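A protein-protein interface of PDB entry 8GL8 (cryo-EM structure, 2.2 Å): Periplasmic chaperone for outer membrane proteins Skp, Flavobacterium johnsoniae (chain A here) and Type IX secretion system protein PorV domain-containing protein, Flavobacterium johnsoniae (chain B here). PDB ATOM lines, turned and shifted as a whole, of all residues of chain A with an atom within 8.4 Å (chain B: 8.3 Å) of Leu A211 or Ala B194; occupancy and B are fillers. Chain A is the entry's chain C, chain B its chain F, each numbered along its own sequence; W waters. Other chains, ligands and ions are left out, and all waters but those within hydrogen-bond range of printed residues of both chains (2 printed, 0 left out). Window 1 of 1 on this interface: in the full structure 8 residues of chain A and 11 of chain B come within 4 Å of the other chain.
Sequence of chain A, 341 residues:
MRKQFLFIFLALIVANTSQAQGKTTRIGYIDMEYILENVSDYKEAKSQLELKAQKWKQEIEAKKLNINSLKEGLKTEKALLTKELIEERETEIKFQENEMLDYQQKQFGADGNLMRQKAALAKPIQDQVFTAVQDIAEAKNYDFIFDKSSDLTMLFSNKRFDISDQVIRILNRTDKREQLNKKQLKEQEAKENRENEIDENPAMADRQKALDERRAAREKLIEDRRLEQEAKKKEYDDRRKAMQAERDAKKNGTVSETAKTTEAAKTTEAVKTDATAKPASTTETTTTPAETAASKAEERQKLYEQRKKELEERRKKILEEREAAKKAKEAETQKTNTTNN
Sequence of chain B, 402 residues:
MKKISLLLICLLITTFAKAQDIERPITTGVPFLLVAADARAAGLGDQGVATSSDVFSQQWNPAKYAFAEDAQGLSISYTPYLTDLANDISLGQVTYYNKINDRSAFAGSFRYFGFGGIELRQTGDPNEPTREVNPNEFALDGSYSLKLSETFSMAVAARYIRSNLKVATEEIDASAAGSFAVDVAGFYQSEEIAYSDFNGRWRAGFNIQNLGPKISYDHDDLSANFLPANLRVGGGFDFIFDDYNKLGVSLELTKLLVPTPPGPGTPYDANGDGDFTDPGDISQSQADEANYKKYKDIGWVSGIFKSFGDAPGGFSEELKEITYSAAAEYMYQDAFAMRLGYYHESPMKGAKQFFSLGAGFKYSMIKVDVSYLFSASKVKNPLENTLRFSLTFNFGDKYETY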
ATOM      1  N   ALA A 203      23.255 -14.340 -18.261  1.00  0.00           N
ATOM      2  CA  ALA A 203      22.357 -13.486 -19.031  1.00  0.00           C
ATOM      3  C   ALA A 203      23.091 -12.299 -19.640  1.00  0.00           C
ATOM      4  O   ALA A 203      22.662 -11.772 -20.673  1.00  0.00           O
ATOM      5  CB  ALA A 203      21.205 -13.004 -18.150  1.00  0.00           C
ATOM      6  N   MET A 204      24.188 -11.861 -19.015  1.00  0.00           N
ATOM      7  CA  MET A 204      24.929 -10.716 -19.532  1.00  0.00           C
ATOM      8  C   MET A 204      25.508 -11.006 -20.911  1.00  0.00           C
ATOM      9  O   MET A 204      25.472 -10.148 -21.800  1.00  0.00           O
ATOM     10  CB  MET A 204      26.038 -10.322 -18.557  1.00  0.00           C
ATOM     11  CG  MET A 204      27.010  -9.294 -19.111  1.00  0.00           C
ATOM     12  SD  MET A 204      28.034  -8.536 -17.838  1.00  0.00           S
ATOM     13  CE  MET A 204      28.763  -7.184 -18.758  1.00  0.00           C
ATOM     14  N   ALA A 205      26.052 -12.210 -21.105  1.00  0.00           N
ATOM     15  CA  ALA A 205      26.599 -12.570 -22.409  1.00  0.00           C
ATOM     16  C   ALA A 205      25.512 -12.594 -23.476  1.00  0.00           C
ATOM     17  O   ALA A 205      25.723 -12.120 -24.599  1.00  0.00           O
ATOM     18  CB  ALA A 205      27.305 -13.924 -22.329  1.00  0.00           C
ATOM     19  N   ASP A 206      24.341 -13.142 -23.142  1.00  0.00           N
ATOM     20  CA  ASP A 206      23.237 -13.166 -24.096  1.00  0.00           C
ATOM     21  C   ASP A 206      22.780 -11.755 -24.447  1.00  0.00           C
ATOM     22  O   ASP A 206      22.520 -11.451 -25.618  1.00  0.00           O
ATOM     23  CB  ASP A 206      22.074 -13.981 -23.529  1.00  0.00           C
ATOM     24  CG  ASP A 206      22.364 -15.467 -23.499  1.00  0.00           C
ATOM     25  OD1 ASP A 206      22.566 -16.058 -24.581  1.00  0.00           O
ATOM     26  OD2 ASP A 206      22.390 -16.047 -22.393  1.00  0.00           O
ATOM     27  N   ARG A 207      22.677 -10.878 -23.445  1.00  0.00           N
ATOM     28  CA  ARG A 207      22.265  -9.503 -23.706  1.00  0.00           C
ATOM     29  C   ARG A 207      23.291  -8.772 -24.565  1.00  0.00           C
ATOM     30  O   ARG A 207      22.926  -8.019 -25.476  1.00  0.00           O
ATOM     31  CB  ARG A 207      22.041  -8.764 -22.388  1.00  0.00           C
ATOM     32  CG  ARG A 207      20.717  -9.090 -21.717  1.00  0.00           C
ATOM     33  CD  ARG A 207      20.454  -8.172 -20.535  1.00  0.00           C
ATOM     34  NE  ARG A 207      20.840  -8.782 -19.270  1.00  0.00           N
ATOM     35  CZ  ARG A 207      21.964  -8.515 -18.620  1.00  0.00           C
ATOM     36  NH1 ARG A 207      22.845  -7.648 -19.092  1.00  0.00           N
ATOM     37  NH2 ARG A 207      22.211  -9.132 -17.468  1.00  0.00           N
ATOM     38  N   GLN A 208      24.580  -8.981 -24.289  1.00  0.00           N
ATOM     39  CA  GLN A 208      25.623  -8.351 -25.093  1.00  0.00           C
ATOM     40  C   GLN A 208      25.591  -8.860 -26.529  1.00  0.00           C
ATOM     41  O   GLN A 208      25.762  -8.084 -27.475  1.00  0.00           O
ATOM     42  CB  GLN A 208      26.991  -8.600 -24.460  1.00  0.00           C
ATOM     43  CG  GLN A 208      28.136  -7.820 -25.090  1.00  0.00           C
ATOM     44  CD  GLN A 208      27.746  -6.404 -25.471  1.00  0.00           C
ATOM     45  OE1 GLN A 208      27.508  -6.106 -26.641  1.00  0.00           O
ATOM     46  NE2 GLN A 208      27.684  -5.522 -24.481  1.00  0.00           N
ATOM     47  N   LYS A 209      25.372 -10.165 -26.710  1.00  0.00           N
ATOM     48  CA  LYS A 209      25.259 -10.716 -28.057  1.00  0.00           C
ATOM     49  C   LYS A 209      24.060 -10.130 -28.790  1.00  0.00           C
ATOM     50  O   LYS A 209      24.147  -9.809 -29.981  1.00  0.00           O
ATOM     51  CB  LYS A 209      25.157 -12.239 -27.996  1.00  0.00           C
ATOM     52  CG  LYS A 209      26.482 -12.948 -27.772  1.00  0.00           C
ATOM     53  CD  LYS A 209      26.341 -14.449 -27.981  1.00  0.00           C
ATOM     54  CE  LYS A 209      27.504 -15.212 -27.368  1.00  0.00           C
ATOM     55  NZ  LYS A 209      28.397 -14.331 -26.565  1.00  0.00           N
ATOM     56  N   ALA A 210      22.928  -9.988 -28.094  1.00  0.00           N
ATOM     57  CA  ALA A 210      21.748  -9.395 -28.716  1.00  0.00           C
ATOM     58  C   ALA A 210      22.005  -7.948 -29.118  1.00  0.00           C
ATOM     59  O   ALA A 210      21.602  -7.517 -30.206  1.00  0.00           O
ATOM     60  CB  ALA A 210      20.553  -9.487 -27.768  1.00  0.00           C
ATOM     61  N   LEU A 211      22.677  -7.183 -28.254  1.00  0.00           N
ATOM     62  CA  LEU A 211      23.001  -5.798 -28.586  1.00  0.00           C
ATOM     63  C   LEU A 211      23.939  -5.722 -29.785  1.00  0.00           C
ATOM     64  O   LEU A 211      23.762  -4.875 -30.669  1.00  0.00           O
ATOM     65  CB  LEU A 211      23.617  -5.095 -27.377  1.00  0.00           C
ATOM     66  CG  LEU A 211      22.687  -4.826 -26.192  1.00  0.00           C
ATOM     67  CD1 LEU A 211      23.450  -4.175 -25.051  1.00  0.00           C
ATOM     68  CD2 LEU A 211      21.511  -3.962 -26.617  1.00  0.00           C
ATOM     69  N   ASP A 212      24.947  -6.597 -29.829  1.00  0.00           N
ATOM     70  CA  ASP A 212      25.869  -6.611 -30.960  1.00  0.00           C
ATOM     71  C   ASP A 212      25.150  -6.968 -32.256  1.00  0.00           C
ATOM     72  O   ASP A 212      25.405  -6.363 -33.306  1.00  0.00           O
ATOM     73  CB  ASP A 212      27.013  -7.590 -30.693  1.00  0.00           C
ATOM     74  CG  ASP A 212      28.145  -6.962 -29.904  1.00  0.00           C
ATOM     75  OD1 ASP A 212      28.349  -5.736 -30.027  1.00  0.00           O
ATOM     76  OD2 ASP A 212      28.831  -7.695 -29.160  1.00  0.00           O
ATOM     77  N   GLU A 213      24.251  -7.954 -32.203  1.00  0.00           N
ATOM     78  CA  GLU A 213      23.490  -8.327 -33.390  1.00  0.00           C
ATOM     79  C   GLU A 213      22.587  -7.189 -33.845  1.00  0.00           C
ATOM     80  O   GLU A 213      22.463  -6.930 -35.048  1.00  0.00           O
ATOM     81  CB  GLU A 213      22.671  -9.588 -33.116  1.00  0.00           C
ATOM     82  CG  GLU A 213      23.486 -10.871 -33.133  1.00  0.00           C
ATOM     83  CD  GLU A 213      23.082 -11.833 -32.035  1.00  0.00           C
ATOM     84  OE1 GLU A 213      21.953 -11.703 -31.517  1.00  0.00           O
ATOM     85  OE2 GLU A 213      23.892 -12.717 -31.689  1.00  0.00           O
ATOM     86  N   ARG A 214      21.945  -6.498 -32.899  1.00  0.00           N
ATOM     87  CA  ARG A 214      21.119  -5.350 -33.255  1.00  0.00           C
ATOM     88  C   ARG A 214      21.952  -4.258 -33.914  1.00  0.00           C
ATOM     89  O   ARG A 214      21.533  -3.666 -34.916  1.00  0.00           O
ATOM     90  CB  ARG A 214      20.414  -4.801 -32.015  1.00  0.00           C
ATOM     91  CG  ARG A 214      19.128  -5.520 -31.648  1.00  0.00           C
ATOM     92  CD  ARG A 214      18.352  -4.737 -30.601  1.00  0.00           C
ATOM     93  NE  ARG A 214      18.331  -5.417 -29.311  1.00  0.00           N
ATOM     94  CZ  ARG A 214      18.244  -4.799 -28.142  1.00  0.00           C
ATOM     95  NH1 ARG A 214      18.171  -3.480 -28.060  1.00  0.00           N
ATOM     96  NH2 ARG A 214      18.230  -5.521 -27.025  1.00  0.00           N
ATOM     97  N   ARG A 215      23.137  -3.980 -33.363  1.00  0.00           N
ATOM     98  CA  ARG A 215      24.006  -2.962 -33.945  1.00  0.00           C
ATOM     99  C   ARG A 215      24.426  -3.340 -35.359  1.00  0.00           C
ATOM    100  O   ARG A 215      24.376  -2.508 -36.274  1.00  0.00           O
ATOM    101  CB  ARG A 215      25.234  -2.754 -33.059  1.00  0.00           C
ATOM    102  CG  ARG A 215      26.328  -1.918 -33.701  1.00  0.00           C
ATOM    103  CD  ARG A 215      26.846  -0.857 -32.744  1.00  0.00           C
ATOM    104  NE  ARG A 215      25.818   0.116 -32.396  1.00  0.00           N
ATOM    105  CZ  ARG A 215      25.534   0.493 -31.157  1.00  0.00           C
ATOM    106  NH1 ARG A 215      26.188  -0.001 -30.118  1.00  0.00           N
ATOM    107  NH2 ARG A 215      24.570   1.385 -30.954  1.00  0.00           N
ATOM    108  N   ALA A 216      24.833  -4.596 -35.559  1.00  0.00           N
ATOM    109  CA  ALA A 216      25.254  -5.034 -36.886  1.00  0.00           C
ATOM    110  C   ALA A 216      24.103  -4.969 -37.882  1.00  0.00           C
ATOM    111  O   ALA A 216      24.282  -4.515 -39.019  1.00  0.00           O
ATOM    112  CB  ALA A 216      25.824  -6.452 -36.815  1.00  0.00           C
ATOM    113  N   ALA A 217      22.910  -5.411 -37.473  1.00  0.00           N
ATOM    114  CA  ALA A 217      21.761  -5.380 -38.369  1.00  0.00           C
ATOM    115  C   ALA A 217      21.377  -3.952 -38.732  1.00  0.00           C
ATOM    116  O   ALA A 217      21.077  -3.659 -39.895  1.00  0.00           O
ATOM    117  CB  ALA A 217      20.578  -6.109 -37.730  1.00  0.00           C
ATOM    118  N   ARG A 218      21.380  -3.046 -37.750  1.00  0.00           N
ATOM    119  CA  ARG A 218      21.022  -1.660 -38.029  1.00  0.00           C
ATOM    120  C   ARG A 218      22.066  -0.986 -38.909  1.00  0.00           C
ATOM    121  O   ARG A 218      21.731  -0.130 -39.737  1.00  0.00           O
ATOM    122  CB  ARG A 218      20.833  -0.893 -36.720  1.00  0.00           C
ATOM    123  CG  ARG A 218      19.407  -0.938 -36.189  1.00  0.00           C
ATOM    124  CD  ARG A 218      19.186   0.071 -35.073  1.00  0.00           C
ATOM    125  NE  ARG A 218      18.567  -0.541 -33.903  1.00  0.00           N
ATOM    126  CZ  ARG A 218      19.147  -0.645 -32.715  1.00  0.00           C
ATOM    127  NH1 ARG A 218      20.364  -0.175 -32.497  1.00  0.00           N
ATOM    128  NH2 ARG A 218      18.488  -1.233 -31.721  1.00  0.00           N
ATOM    129  N   GLU B 191      24.970   4.569 -26.295  1.00  0.00           N
ATOM    130  CA  GLU B 191      24.251   3.390 -26.740  1.00  0.00           C
ATOM    131  C   GLU B 191      23.947   2.483 -25.550  1.00  0.00           C
ATOM    132  O   GLU B 191      24.451   2.675 -24.440  1.00  0.00           O
ATOM    133  CB  GLU B 191      25.060   2.640 -27.799  1.00  0.00           C
ATOM    134  CG  GLU B 191      26.137   1.726 -27.233  1.00  0.00           C
ATOM    135  CD  GLU B 191      27.322   2.488 -26.668  1.00  0.00           C
ATOM    136  OE1 GLU B 191      27.442   3.700 -26.941  1.00  0.00           O
ATOM    137  OE2 GLU B 191      28.135   1.871 -25.950  1.00  0.00           O
ATOM    138  N   GLU B 192      23.100   1.484 -25.787  1.00  0.00           N
ATOM    139  CA  GLU B 192      22.773   0.526 -24.741  1.00  0.00           C
ATOM    140  C   GLU B 192      24.009  -0.286 -24.373  1.00  0.00           C
ATOM    141  O   GLU B 192      24.677  -0.850 -25.245  1.00  0.00           O
ATOM    142  CB  GLU B 192      21.645  -0.394 -25.200  1.00  0.00           C
ATOM    143  CG  GLU B 192      20.870  -1.044 -24.068  1.00  0.00           C
ATOM    144  CD  GLU B 192      19.554  -1.635 -24.531  1.00  0.00           C
ATOM    145  OE1 GLU B 192      18.993  -1.128 -25.524  1.00  0.00           O
ATOM    146  OE2 GLU B 192      19.082  -2.605 -23.906  1.00  0.00           O
ATOM    147  N   ILE B 193      24.312  -0.344 -23.079  1.00  0.00           N
ATOM    148  CA  ILE B 193      25.501  -1.016 -22.568  1.00  0.00           C
ATOM    149  C   ILE B 193      25.048  -2.097 -21.599  1.00  0.00           C
ATOM    150  O   ILE B 193      24.339  -1.807 -20.628  1.00  0.00           O
ATOM    151  CB  ILE B 193      26.461  -0.033 -21.882  1.00  0.00           C
ATOM    152  CG1 ILE B 193      26.982   0.993 -22.890  1.00  0.00           C
ATOM    153  CG2 ILE B 193      27.613  -0.780 -21.231  1.00  0.00           C
ATOM    154  CD1 ILE B 193      27.346   2.321 -22.274  1.00  0.00           C
ATOM    155  N   ALA B 194      25.469  -3.333 -21.851  1.00  0.00           N
ATOM    156  CA  ALA B 194      25.065  -4.459 -21.020  1.00  0.00           C
ATOM    157  C   ALA B 194      25.917  -4.526 -19.759  1.00  0.00           C
ATOM    158  O   ALA B 194      27.143  -4.397 -19.818  1.00  0.00           O
ATOM    159  CB  ALA B 194      25.175  -5.765 -21.804  1.00  0.00           C
ATOM    160  N   TYR B 195      25.264  -4.723 -18.620  1.00  0.00           N
ATOM    161  CA  TYR B 195      25.925  -4.903 -17.336  1.00  0.00           C
ATOM    162  C   TYR B 195      25.520  -6.260 -16.756  1.00  0.00           C
ATOM    163  O   TYR B 195      24.876  -7.076 -17.421  1.00  0.00           O
ATOM    164  CB  TYR B 195      25.592  -3.750 -16.385  1.00  0.00           C
ATOM    165  CG  TYR B 195      26.052  -2.398 -16.880  1.00  0.00           C
ATOM    166  CD1 TYR B 195      27.373  -1.998 -16.739  1.00  0.00           C
ATOM    167  CD2 TYR B 195      25.164  -1.520 -17.488  1.00  0.00           C
ATOM    168  CE1 TYR B 195      27.799  -0.765 -17.190  1.00  0.00           C
ATOM    169  CE2 TYR B 195      25.581  -0.283 -17.942  1.00  0.00           C
ATOM    170  CZ  TYR B 195      26.899   0.089 -17.790  1.00  0.00           C
ATOM    171  OH  TYR B 195      27.320   1.318 -18.240  1.00  0.00           O
ATOM    172  N   SER B 196      25.912  -6.497 -15.501  1.00  0.00           N
ATOM    173  CA  SER B 196      25.694  -7.803 -14.887  1.00  0.00           C
ATOM    174  C   SER B 196      24.209  -8.129 -14.757  1.00  0.00           C
ATOM    175  O   SER B 196      23.787  -9.254 -15.047  1.00  0.00           O
ATOM    176  CB  SER B 196      26.374  -7.858 -13.520  1.00  0.00           C
ATOM    177  OG  SER B 196      27.583  -7.119 -13.524  1.00  0.00           O
ATOM    178  N   ASP B 197      23.401  -7.162 -14.322  1.00  0.00           N
ATOM    179  CA  ASP B 197      21.991  -7.403 -14.058  1.00  0.00           C
ATOM    180  C   ASP B 197      21.047  -6.667 -14.997  1.00  0.00           C
ATOM    181  O   ASP B 197      19.849  -6.973 -15.003  1.00  0.00           O
ATOM    182  CB  ASP B 197      21.645  -7.020 -12.609  1.00  0.00           C
ATOM    183  CG  ASP B 197      22.583  -7.654 -11.602  1.00  0.00           C
ATOM    184  OD1 ASP B 197      22.328  -8.806 -11.194  1.00  0.00           O
ATOM    185  OD2 ASP B 197      23.576  -7.000 -11.219  1.00  0.00           O
ATOM    186  N   PHE B 198      21.540  -5.713 -15.779  1.00  0.00           N
ATOM    187  CA  PHE B 198      20.698  -4.925 -16.668  1.00  0.00           C
ATOM    188  C   PHE B 198      21.578  -4.342 -17.760  1.00  0.00           C
ATOM    189  O   PHE B 198      22.800  -4.275 -17.623  1.00  0.00           O
ATOM    190  CB  PHE B 198      19.969  -3.813 -15.905  1.00  0.00           C
ATOM    191  CG  PHE B 198      20.819  -3.139 -14.867  1.00  0.00           C
ATOM    192  CD1 PHE B 198      21.712  -2.142 -15.221  1.00  0.00           C
ATOM    193  CD2 PHE B 198      20.733  -3.509 -13.536  1.00  0.00           C
ATOM    194  CE1 PHE B 198      22.498  -1.525 -14.268  1.00  0.00           C
ATOM    195  CE2 PHE B 198      21.516  -2.895 -12.580  1.00  0.00           C
ATOM    196  CZ  PHE B 198      22.400  -1.902 -12.947  1.00  0.00           C
ATOM    197  N   ASN B 199      20.947  -3.920 -18.848  1.00  0.00           N
ATOM    198  CA  ASN B 199      21.646  -3.251 -19.941  1.00  0.00           C
ATOM    199  C   ASN B 199      21.129  -1.816 -20.003  1.00  0.00           C
ATOM    200  O   ASN B 199      20.185  -1.512 -20.731  1.00  0.00           O
ATOM    201  CB  ASN B 199      21.455  -3.987 -21.268  1.00  0.00           C
ATOM    202  CG  ASN B 199      20.029  -4.431 -21.489  1.00  0.00           C
ATOM    203  OD1 ASN B 199      19.180  -4.288 -20.612  1.00  0.00           O
ATOM    204  ND2 ASN B 199      19.757  -4.975 -22.668  1.00  0.00           N
ATOM    205  N   GLY B 200      21.764  -0.932 -19.235  1.00  0.00           N
ATOM    206  CA  GLY B 200      21.327   0.441 -19.112  1.00  0.00           C
ATOM    207  C   GLY B 200      21.892   1.348 -20.188  1.00  0.00           C
ATOM    208  O   GLY B 200      22.553   0.916 -21.134  1.00  0.00           O
ATOM    209  N   ARG B 201      21.614   2.641 -20.030  1.00  0.00           N
ATOM    210  CA  ARG B 201      22.066   3.660 -20.968  1.00  0.00           C
ATOM    211  C   ARG B 201      22.449   4.915 -20.196  1.00  0.00           C
ATOM    212  O   ARG B 201      21.907   5.183 -19.124  1.00  0.00           O
ATOM    213  CB  ARG B 201      20.978   3.975 -22.008  1.00  0.00           C
ATOM    214  CG  ARG B 201      21.424   4.882 -23.138  1.00  0.00           C
ATOM    215  CD  ARG B 201      20.238   5.389 -23.942  1.00  0.00           C
ATOM    216  NE  ARG B 201      19.510   4.302 -24.587  1.00  0.00           N
ATOM    217  CZ  ARG B 201      19.763   3.854 -25.809  1.00  0.00           C
ATOM    218  NH1 ARG B 201      20.722   4.379 -26.553  1.00  0.00           N
ATOM    219  NH2 ARG B 201      19.034   2.854 -26.296  1.00  0.00           N
ATOM    220  N   PHE B 237      20.729   7.868 -15.959  1.00  0.00           N
ATOM    221  CA  PHE B 237      21.007   6.479 -16.286  1.00  0.00           C
ATOM    222  C   PHE B 237      19.699   5.713 -16.420  1.00  0.00           C
ATOM    223  O   PHE B 237      18.765   5.913 -15.641  1.00  0.00           O
ATOM    224  CB  PHE B 237      21.895   5.817 -15.226  1.00  0.00           C
ATOM    225  CG  PHE B 237      22.248   4.394 -15.541  1.00  0.00           C
ATOM    226  CD1 PHE B 237      23.250   4.101 -16.449  1.00  0.00           C
ATOM    227  CD2 PHE B 237      21.572   3.349 -14.937  1.00  0.00           C
ATOM    228  CE1 PHE B 237      23.576   2.794 -16.745  1.00  0.00           C
ATOM    229  CE2 PHE B 237      21.894   2.039 -15.230  1.00  0.00           C
ATOM    230  CZ  PHE B 237      22.897   1.762 -16.134  1.00  0.00           C
ATOM    231  N   ILE B 240      17.476  -0.888 -17.792  1.00  0.00           N
ATOM    232  CA  ILE B 240      16.556  -1.565 -18.699  1.00  0.00           C
ATOM    233  C   ILE B 240      16.515  -3.036 -18.309  1.00  0.00           C
ATOM    234  O   ILE B 240      17.520  -3.746 -18.430  1.00  0.00           O
ATOM    235  CB  ILE B 240      16.967  -1.385 -20.167  1.00  0.00           C
ATOM    236  CG1 ILE B 240      16.908   0.093 -20.554  1.00  0.00           C
ATOM    237  CG2 ILE B 240      16.070  -2.210 -21.074  1.00  0.00           C
ATOM    238  CD1 ILE B 240      17.992   0.536 -21.506  1.00  0.00           C
ATOM    239  N   TYR B 402      20.352   4.736 -31.797  1.00  0.00           N
ATOM    240  CA  TYR B 402      21.682   4.141 -31.756  1.00  0.00           C
ATOM    241  C   TYR B 402      22.048   3.739 -30.331  1.00  0.00           C
ATOM    242  O   TYR B 402      21.604   2.705 -29.832  1.00  0.00           O
ATOM    243  CB  TYR B 402      22.717   5.116 -32.322  1.00  0.00           C
ATOM    244  CG  TYR B 402      24.157   4.686 -32.144  1.00  0.00           C
ATOM    245  CD1 TYR B 402      24.783   3.883 -33.087  1.00  0.00           C
ATOM    246  CD2 TYR B 402      24.897   5.101 -31.043  1.00  0.00           C
ATOM    247  CE1 TYR B 402      26.099   3.494 -32.933  1.00  0.00           C
ATOM    248  CE2 TYR B 402      26.212   4.715 -30.881  1.00  0.00           C
ATOM    249  CZ  TYR B 402      26.808   3.913 -31.829  1.00  0.00           C
ATOM    250  OH  TYR B 402      28.120   3.528 -31.671  1.00  0.00           O
HETATM  251  O   HOH W   1      19.355  -7.104 -25.060  1.00  0.00           O
HETATM  252  O   HOH W   2      19.547   0.312 -29.304  1.00  0.00           O
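O of Tyr B402 lies close to NH2 of Arg A215. The guanidinium group (NH2) of Arg A207 sits at hydrogen-bond distance from the backbone carbonyl oxygen (O) of Ser B196, at 2.9 Å. The side-chain carboxylate (OE1) of Glu B192 lies within salt-bridge range of the guanidinium group (NH1) of Arg A214 (3.6 Å). The guanidinium group of Arg A207 is in hydrogen-bond range of the backbone carbonyl oxygen of Tyr B195 (2.7 Å). The side-chain sulfur (SD) of Met A204 sits close to the backbone carbonyl oxygen (O) of Tyr B195 (3.5 Å). The side-chain sulfur (SD) of Met A204 is in hydrogen-bond range of the backbone NH (N) of Ser B196.
The side-chain amide oxygen (OD1) of Asn B199 sits close to the backbone carbonyl oxygen (O) of Ile B240 (2.8 Å). The side-chain amide nitrogen (ND2) of Asn B199 is in hydrogen-bond range of the side-chain carboxylate (OE2) of Glu B192 (2.8 Å). OE1 of Gln A208 lies close to OD2 of Asp A212 (3.3 Å).
Ala B194 touches Met A204 (O to CE, 3.4 Å). Asp B197 touches Arg A207 (C to NH2, 3.7 Å). Arg A207 touches Phe B198 (NH1 to O, 3.7 Å). CG of Asn B199 touches CD of Arg A207, at 3.9 Å. Ala B194 touches Gln A208 (CB to NE2, 3.7 Å). Glu B192 touches Leu A211 (O to CD1, 3.5 Å). Leu A211 touches Ala B194 (CD1 to N, 3.9 Å). CG of Glu B191 touches NH1 of Arg A215, 3.4 Å away.
Of chain B, only Glu B192 (3.5 Å) and Ala B194 (3.9 Å) come within 4 Å of Leu A211. Ala B194 touches just these residues of chain A: Met A204, Gln A208 and Leu A211. Of the printed residues of chain A, Ser B196 touches Met A204 and Arg A207. Printed residues of chain B within 4 Å of Met A204: Ala B194, Tyr B195 and Ser B196. The nearest printed residue of chain A that does not touch Tyr B195 is Ala A203 (5.9 Å).
Of the 16 printed residues of chain A, 6 touch a printed residue of chain B. Of the 14 printed residues of chain B, 9 touch a printed residue of chain A. Among the printed residues, 14 pairs touch across the chains. Among the printed residues, Asp or Glu carboxylates within 4 Å of a Lys or Arg side-chain nitrogen of the other chain: Arg A214 with Glu B192 (3.6 Å).
Water W1 bridges NH2 of Arg A214 (2.8 Å) and ND2 of Asn B199 (3.2 Å). Water W2 lies within hydrogen-bond range of the guanidinium group of Arg A218 (3.1 Å) and the backbone carbonyl oxygen of Tyr B402 (3.2 Å).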
